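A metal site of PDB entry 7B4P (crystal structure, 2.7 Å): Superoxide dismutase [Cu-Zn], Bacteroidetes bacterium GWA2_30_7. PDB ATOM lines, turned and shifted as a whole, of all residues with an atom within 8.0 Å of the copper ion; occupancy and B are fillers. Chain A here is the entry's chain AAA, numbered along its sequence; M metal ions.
A ring nitrogen (ND1) of His 53 is in hydrogen-bond range of the backbone carbonyl oxygen (O) of Gly 67, at 2.8 Å. The backbone NH (N) of His 126 lies within hydrogen-bond range of the backbone carbonyl oxygen (O) of Gly 49. ND1 of His 53 lies close to O of Gly 68. O of His 51 lies within hydrogen-bond range of N of Ile 124 (3.0 Å). A ring nitrogen (ND1) of His 126 lies within hydrogen-bond range of the backbone carbonyl oxygen (O) of Gly 141 (3.0 Å). A ring nitrogen (NE2) of His 51 lies within hydrogen-bond range of the side-chain carboxylate (OD2) of Asp 130, at 2.7 Å. A ring nitrogen (ND1) of His 51 sits close to a ring nitrogen (NE2) of His 69 (3.3 Å). The backbone carbonyl oxygen (O) of Ser 122 is in hydrogen-bond range of the backbone NH (N) of His 53, 2.7 Å away.
His 69 touches the copper ion. Along chain A the residues within 4 Å of the copper ion span positions 51 to 126. The nearest printed residue that does not touch the copper ion is Ile 124 (4.1 Å).
The copper ion is bound by NE2 of His 126 (2.1 Å), NE2 of His 53 (2.1 Å) and ND1 of His 51 (2.2 Å). The copper ion has three donor atoms within binding distance.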
ATOM      1  N   GLY A  49      24.435  24.709  23.591  1.00  0.00           N
ATOM      2  CA  GLY A  49      24.980  23.356  23.785  1.00  0.00           C
ATOM      3  C   GLY A  49      26.475  23.333  23.511  1.00  0.00           C
ATOM      4  O   GLY A  49      26.908  23.891  22.491  1.00  0.00           O
ATOM      5  N   PHE A  50      27.228  22.705  24.420  1.00  0.00           N
ATOM      6  CA  PHE A  50      28.712  22.711  24.468  1.00  0.00           C
ATOM      7  C   PHE A  50      29.185  21.305  24.833  1.00  0.00           C
ATOM      8  O   PHE A  50      29.055  20.914  26.017  1.00  0.00           O
ATOM      9  CB  PHE A  50      29.158  23.785  25.465  1.00  0.00           C
ATOM     10  CG  PHE A  50      30.633  24.121  25.473  1.00  0.00           C
ATOM     11  CD1 PHE A  50      31.238  24.729  24.383  1.00  0.00           C
ATOM     12  CD2 PHE A  50      31.403  23.879  26.600  1.00  0.00           C
ATOM     13  CE1 PHE A  50      32.581  25.050  24.411  1.00  0.00           C
ATOM     14  CE2 PHE A  50      32.754  24.199  26.620  1.00  0.00           C
ATOM     15  CZ  PHE A  50      33.338  24.780  25.530  1.00  0.00           C
ATOM     16  N   HIS A  51      29.682  20.542  23.847  1.00  0.00           N
ATOM     17  CA  HIS A  51      29.986  19.087  23.977  1.00  0.00           C
ATOM     18  C   HIS A  51      31.297  18.731  23.277  1.00  0.00           C
ATOM     19  O   HIS A  51      31.693  19.446  22.337  1.00  0.00           O
ATOM     20  CB  HIS A  51      28.839  18.250  23.388  1.00  0.00           C
ATOM     21  CG  HIS A  51      27.476  18.627  23.850  1.00  0.00           C
ATOM     22  ND1 HIS A  51      26.474  18.977  22.961  1.00  0.00           N
ATOM     23  CD2 HIS A  51      26.936  18.704  25.079  1.00  0.00           C
ATOM     24  CE1 HIS A  51      25.379  19.261  23.632  1.00  0.00           C
ATOM     25  NE2 HIS A  51      25.633  19.094  24.937  1.00  0.00           N
ATOM     26  N   ILE A  52      31.930  17.635  23.728  1.00  0.00           N
ATOM     27  CA  ILE A  52      33.005  16.909  22.992  1.00  0.00           C
ATOM     28  C   ILE A  52      32.337  15.780  22.195  1.00  0.00           C
ATOM     29  O   ILE A  52      31.621  14.969  22.812  1.00  0.00           O
ATOM     30  CB  ILE A  52      34.079  16.387  23.969  1.00  0.00           C
ATOM     31  CG1 ILE A  52      34.769  17.524  24.731  1.00  0.00           C
ATOM     32  CG2 ILE A  52      35.081  15.502  23.243  1.00  0.00           C
ATOM     33  CD1 ILE A  52      35.544  17.062  25.945  1.00  0.00           C
ATOM     34  N   HIS A  53      32.554  15.740  20.877  1.00  0.00           N
ATOM     35  CA  HIS A  53      31.968  14.743  19.948  1.00  0.00           C
ATOM     36  C   HIS A  53      33.049  13.715  19.565  1.00  0.00           C
ATOM     37  O   HIS A  53      34.241  14.065  19.630  1.00  0.00           O
ATOM     38  CB  HIS A  53      31.341  15.440  18.738  1.00  0.00           C
ATOM     39  CG  HIS A  53      30.063  16.143  19.058  1.00  0.00           C
ATOM     40  ND1 HIS A  53      28.891  15.865  18.371  1.00  0.00           N
ATOM     41  CD2 HIS A  53      29.760  17.073  19.978  1.00  0.00           C
ATOM     42  CE1 HIS A  53      27.922  16.621  18.862  1.00  0.00           C
ATOM     43  NE2 HIS A  53      28.424  17.368  19.847  1.00  0.00           N
ATOM     44  N   ALA A  66      31.540  15.606  12.797  1.00  0.00           N
ATOM     45  CA  ALA A  66      31.968  15.452  14.199  1.00  0.00           C
ATOM     46  C   ALA A  66      31.314  14.219  14.835  1.00  0.00           C
ATOM     47  O   ALA A  66      31.855  13.702  15.823  1.00  0.00           O
ATOM     48  CB  ALA A  66      31.648  16.698  14.981  1.00  0.00           C
ATOM     49  N   GLY A  67      30.182  13.776  14.272  1.00  0.00           N
ATOM     50  CA  GLY A  67      29.429  12.600  14.759  1.00  0.00           C
ATOM     51  C   GLY A  67      28.720  12.892  16.064  1.00  0.00           C
ATOM     52  O   GLY A  67      28.435  14.071  16.337  1.00  0.00           O
ATOM     53  N   GLY A  68      28.436  11.845  16.839  1.00  0.00           N
ATOM     54  CA  GLY A  68      27.691  11.932  18.114  1.00  0.00           C
ATOM     55  C   GLY A  68      28.567  12.403  19.251  1.00  0.00           C
ATOM     56  O   GLY A  68      29.774  12.618  19.039  1.00  0.00           O
ATOM     57  N   HIS A  69      27.968  12.555  20.444  1.00  0.00           N
ATOM     58  CA  HIS A  69      28.647  12.937  21.713  1.00  0.00           C
ATOM     59  C   HIS A  69      29.666  11.850  22.074  1.00  0.00           C
ATOM     60  O   HIS A  69      29.289  10.663  22.010  1.00  0.00           O
ATOM     61  CB  HIS A  69      27.609  13.161  22.818  1.00  0.00           C
ATOM     62  CG  HIS A  69      26.714  14.330  22.582  1.00  0.00           C
ATOM     63  ND1 HIS A  69      25.990  14.923  23.605  1.00  0.00           N
ATOM     64  CD2 HIS A  69      26.418  15.029  21.463  1.00  0.00           C
ATOM     65  CE1 HIS A  69      25.288  15.932  23.118  1.00  0.00           C
ATOM     66  NE2 HIS A  69      25.544  16.017  21.805  1.00  0.00           N
ATOM     67  N   PHE A  70      30.884  12.244  22.424  1.00  0.00           N
ATOM     68  CA  PHE A  70      31.982  11.323  22.833  1.00  0.00           C
ATOM     69  C   PHE A  70      31.527  10.546  24.077  1.00  0.00           C
ATOM     70  O   PHE A  70      31.588  11.100  25.195  1.00  0.00           O
ATOM     71  CB  PHE A  70      33.283  12.093  23.071  1.00  0.00           C
ATOM     72  CG  PHE A  70      34.453  11.238  23.494  1.00  0.00           C
ATOM     73  CD1 PHE A  70      34.784  10.099  22.788  1.00  0.00           C
ATOM     74  CD2 PHE A  70      35.223  11.589  24.594  1.00  0.00           C
ATOM     75  CE1 PHE A  70      35.855   9.306  23.169  1.00  0.00           C
ATOM     76  CE2 PHE A  70      36.295  10.797  24.975  1.00  0.00           C
ATOM     77  CZ  PHE A  70      36.612   9.660  24.270  1.00  0.00           C
ATOM     78  N   HIS A  77      22.840  10.814  28.150  1.00  0.00           N
ATOM     79  CA  HIS A  77      23.139  12.267  28.097  1.00  0.00           C
ATOM     80  C   HIS A  77      22.731  12.906  29.419  1.00  0.00           C
ATOM     81  O   HIS A  77      21.660  12.558  29.943  1.00  0.00           O
ATOM     82  CB  HIS A  77      22.427  12.929  26.911  1.00  0.00           C
ATOM     83  CG  HIS A  77      22.642  14.399  26.834  1.00  0.00           C
ATOM     84  ND1 HIS A  77      23.835  14.944  26.392  1.00  0.00           N
ATOM     85  CD2 HIS A  77      21.857  15.442  27.154  1.00  0.00           C
ATOM     86  CE1 HIS A  77      23.758  16.254  26.428  1.00  0.00           C
ATOM     87  NE2 HIS A  77      22.553  16.589  26.902  1.00  0.00           N
ATOM     88  N   GLY A  88      31.878  13.638  27.076  1.00  0.00           N
ATOM     89  CA  GLY A  88      31.838  14.949  26.409  1.00  0.00           C
ATOM     90  C   GLY A  88      30.558  15.726  26.689  1.00  0.00           C
ATOM     91  O   GLY A  88      30.103  16.437  25.777  1.00  0.00           O
ATOM     92  N   ASP A  89      30.008  15.612  27.908  1.00  0.00           N
ATOM     93  CA  ASP A  89      28.866  16.444  28.383  1.00  0.00           C
ATOM     94  C   ASP A  89      29.418  17.594  29.224  1.00  0.00           C
ATOM     95  O   ASP A  89      29.505  17.444  30.459  1.00  0.00           O
ATOM     96  CB  ASP A  89      27.836  15.608  29.157  1.00  0.00           C
ATOM     97  CG  ASP A  89      26.900  14.791  28.282  1.00  0.00           C
ATOM     98  OD1 ASP A  89      26.953  14.954  27.047  1.00  0.00           O
ATOM     99  OD2 ASP A  89      26.120  14.005  28.840  1.00  0.00           O
ATOM    100  N   GLY A  91      27.923  20.515  29.306  1.00  0.00           N
ATOM    101  CA  GLY A  91      26.718  21.317  29.570  1.00  0.00           C
ATOM    102  C   GLY A  91      26.503  22.404  28.524  1.00  0.00           C
ATOM    103  O   GLY A  91      26.563  22.085  27.320  1.00  0.00           O
ATOM    104  N   SER A 122      36.469  16.242  18.874  1.00  0.00           N
ATOM    105  CA  SER A 122      35.965  17.557  18.399  1.00  0.00           C
ATOM    106  C   SER A 122      35.157  18.245  19.510  1.00  0.00           C
ATOM    107  O   SER A 122      34.500  17.538  20.286  1.00  0.00           O
ATOM    108  CB  SER A 122      35.132  17.409  17.150  1.00  0.00           C
ATOM    109  OG  SER A 122      34.067  16.492  17.354  1.00  0.00           O
ATOM    110  N   MET A 123      35.259  19.579  19.581  1.00  0.00           N
ATOM    111  CA  MET A 123      34.323  20.461  20.324  1.00  0.00           C
ATOM    112  C   MET A 123      33.235  20.914  19.345  1.00  0.00           C
ATOM    113  O   MET A 123      33.589  21.288  18.213  1.00  0.00           O
ATOM    114  CB  MET A 123      35.041  21.692  20.884  1.00  0.00           C
ATOM    115  CG  MET A 123      35.945  21.410  22.080  1.00  0.00           C
ATOM    116  SD  MET A 123      35.058  20.833  23.547  1.00  0.00           S
ATOM    117  CE  MET A 123      33.697  21.991  23.624  1.00  0.00           C
ATOM    118  N   ILE A 124      31.975  20.874  19.767  1.00  0.00           N
ATOM    119  CA  ILE A 124      30.796  21.357  18.985  1.00  0.00           C
ATOM    120  C   ILE A 124      29.993  22.330  19.848  1.00  0.00           C
ATOM    121  O   ILE A 124      29.647  21.954  20.987  1.00  0.00           O
ATOM    122  CB  ILE A 124      29.927  20.185  18.486  1.00  0.00           C
ATOM    123  CG1 ILE A 124      30.643  19.340  17.436  1.00  0.00           C
ATOM    124  CG2 ILE A 124      28.570  20.662  17.989  1.00  0.00           C
ATOM    125  CD1 ILE A 124      30.817  20.034  16.102  1.00  0.00           C
ATOM    126  N   VAL A 125      29.724  23.529  19.327  1.00  0.00           N
ATOM    127  CA  VAL A 125      28.776  24.511  19.914  1.00  0.00           C
ATOM    128  C   VAL A 125      27.470  24.429  19.109  1.00  0.00           C
ATOM    129  O   VAL A 125      27.549  24.435  17.865  1.00  0.00           O
ATOM    130  CB  VAL A 125      29.355  25.936  19.923  1.00  0.00           C
ATOM    131  CG1 VAL A 125      28.459  26.901  20.691  1.00  0.00           C
ATOM    132  CG2 VAL A 125      30.774  25.965  20.486  1.00  0.00           C
ATOM    133  N   HIS A 126      26.334  24.322  19.798  1.00  0.00           N
ATOM    134  CA  HIS A 126      24.984  24.139  19.196  1.00  0.00           C
ATOM    135  C   HIS A 126      24.263  25.481  19.116  1.00  0.00           C
ATOM    136  O   HIS A 126      24.672  26.410  19.846  1.00  0.00           O
ATOM    137  CB  HIS A 126      24.188  23.092  19.975  1.00  0.00           C
ATOM    138  CG  HIS A 126      24.744  21.709  19.862  1.00  0.00           C
ATOM    139  ND1 HIS A 126      24.330  20.822  18.894  1.00  0.00           N
ATOM    140  CD2 HIS A 126      25.700  21.069  20.576  1.00  0.00           C
ATOM    141  CE1 HIS A 126      24.993  19.683  19.030  1.00  0.00           C
ATOM    142  NE2 HIS A 126      25.839  19.818  20.051  1.00  0.00           N
ATOM    143  N   ASP A 130      21.172  23.162  25.480  1.00  0.00           N
ATOM    144  CA  ASP A 130      21.154  21.739  25.925  1.00  0.00           C
ATOM    145  C   ASP A 130      20.345  21.673  27.231  1.00  0.00           C
ATOM    146  O   ASP A 130      20.835  22.196  28.247  1.00  0.00           O
ATOM    147  CB  ASP A 130      22.574  21.202  26.082  1.00  0.00           C
ATOM    148  CG  ASP A 130      22.675  19.819  26.694  1.00  0.00           C
ATOM    149  OD1 ASP A 130      21.619  19.195  26.919  1.00  0.00           O
ATOM    150  OD2 ASP A 130      23.807  19.367  26.948  1.00  0.00           O
ATOM    151  N   PRO A 136      19.244  11.667  22.537  1.00  0.00           N
ATOM    152  CA  PRO A 136      20.553  11.592  23.178  1.00  0.00           C
ATOM    153  C   PRO A 136      21.349  12.912  23.178  1.00  0.00           C
ATOM    154  O   PRO A 136      22.509  12.888  23.573  1.00  0.00           O
ATOM    155  CB  PRO A 136      21.242  10.573  22.262  1.00  0.00           C
ATOM    156  CG  PRO A 136      20.740  10.936  20.873  1.00  0.00           C
ATOM    157  CD  PRO A 136      19.330  11.445  21.089  1.00  0.00           C
ATOM    158  N   THR A 137      20.726  14.015  22.748  1.00  0.00           N
ATOM    159  CA  THR A 137      21.398  15.294  22.377  1.00  0.00           C
ATOM    160  C   THR A 137      21.114  16.390  23.411  1.00  0.00           C
ATOM    161  O   THR A 137      21.966  17.296  23.543  1.00  0.00           O
ATOM    162  CB  THR A 137      20.944  15.749  20.991  1.00  0.00           C
ATOM    163  OG1 THR A 137      19.523  15.800  20.978  1.00  0.00           O
ATOM    164  CG2 THR A 137      21.423  14.821  19.891  1.00  0.00           C
ATOM    165  N   GLY A 138      19.974  16.335  24.103  1.00  0.00           N
ATOM    166  CA  GLY A 138      19.469  17.421  24.971  1.00  0.00           C
ATOM    167  C   GLY A 138      18.722  18.482  24.169  1.00  0.00           C
ATOM    168  O   GLY A 138      18.539  19.590  24.689  1.00  0.00           O
ATOM    169  N   ALA A 140      19.631  20.192  21.632  1.00  0.00           N
ATOM    170  CA  ALA A 140      20.544  21.336  21.383  1.00  0.00           C
ATOM    171  C   ALA A 140      20.398  21.833  19.942  1.00  0.00           C
ATOM    172  O   ALA A 140      20.654  23.017  19.699  1.00  0.00           O
ATOM    173  CB  ALA A 140      21.968  20.925  21.689  1.00  0.00           C
ATOM    174  N   GLY A 141      20.021  20.937  19.021  1.00  0.00           N
ATOM    175  CA  GLY A 141      19.735  21.267  17.613  1.00  0.00           C
ATOM    176  C   GLY A 141      21.007  21.414  16.785  1.00  0.00           C
ATOM    177  O   GLY A 141      21.991  20.714  17.076  1.00  0.00           O
ATOM    178  N   ALA A 142      20.976  22.319  15.791  1.00  0.00           N
ATOM    179  CA  ALA A 142      22.011  22.501  14.750  1.00  0.00           C
ATOM    180  C   ALA A 142      23.349  22.900  15.392  1.00  0.00           C
ATOM    181  O   ALA A 142      23.342  23.478  16.499  1.00  0.00           O
ATOM    182  CB  ALA A 142      21.555  23.553  13.763  1.00  0.00           C
ATOM    183  N   ARG A 143      24.446  22.596  14.698  1.00  0.00           N
ATOM    184  CA  ARG A 143      25.842  22.880  15.126  1.00  0.00           C
ATOM    185  C   ARG A 143      26.306  24.183  14.461  1.00  0.00           C
ATOM    186  O   ARG A 143      26.219  24.262  13.222  1.00  0.00           O
ATOM    187  CB  ARG A 143      26.733  21.684  14.786  1.00  0.00           C
ATOM    188  CG  ARG A 143      26.174  20.357  15.277  1.00  0.00           C
ATOM    189  CD  ARG A 143      26.945  19.139  14.822  1.00  0.00           C
ATOM    190  NE  ARG A 143      26.316  17.928  15.315  1.00  0.00           N
ATOM    191  CZ  ARG A 143      26.824  16.697  15.219  1.00  0.00           C
ATOM    192  NH1 ARG A 143      28.001  16.506  14.634  1.00  0.00           N
ATOM    193  NH2 ARG A 143      26.161  15.676  15.724  1.00  0.00           N
ATOM    194  N   ALA A 145      29.418  25.826  15.399  1.00  0.00           N
ATOM    195  CA  ALA A 145      30.901  25.846  15.376  1.00  0.00           C
ATOM    196  C   ALA A 145      31.456  24.446  15.667  1.00  0.00           C
ATOM    197  O   ALA A 145      30.816  23.686  16.410  1.00  0.00           O
ATOM    198  CB  ALA A 145      31.428  26.862  16.360  1.00  0.00           C
HETATM  199 CU    CU M   1      27.000  18.373  20.947  1.00  0.00          CU
HETATM  200 ZN    ZN M   2      25.879  14.033  25.422  1.00  0.00          ZN
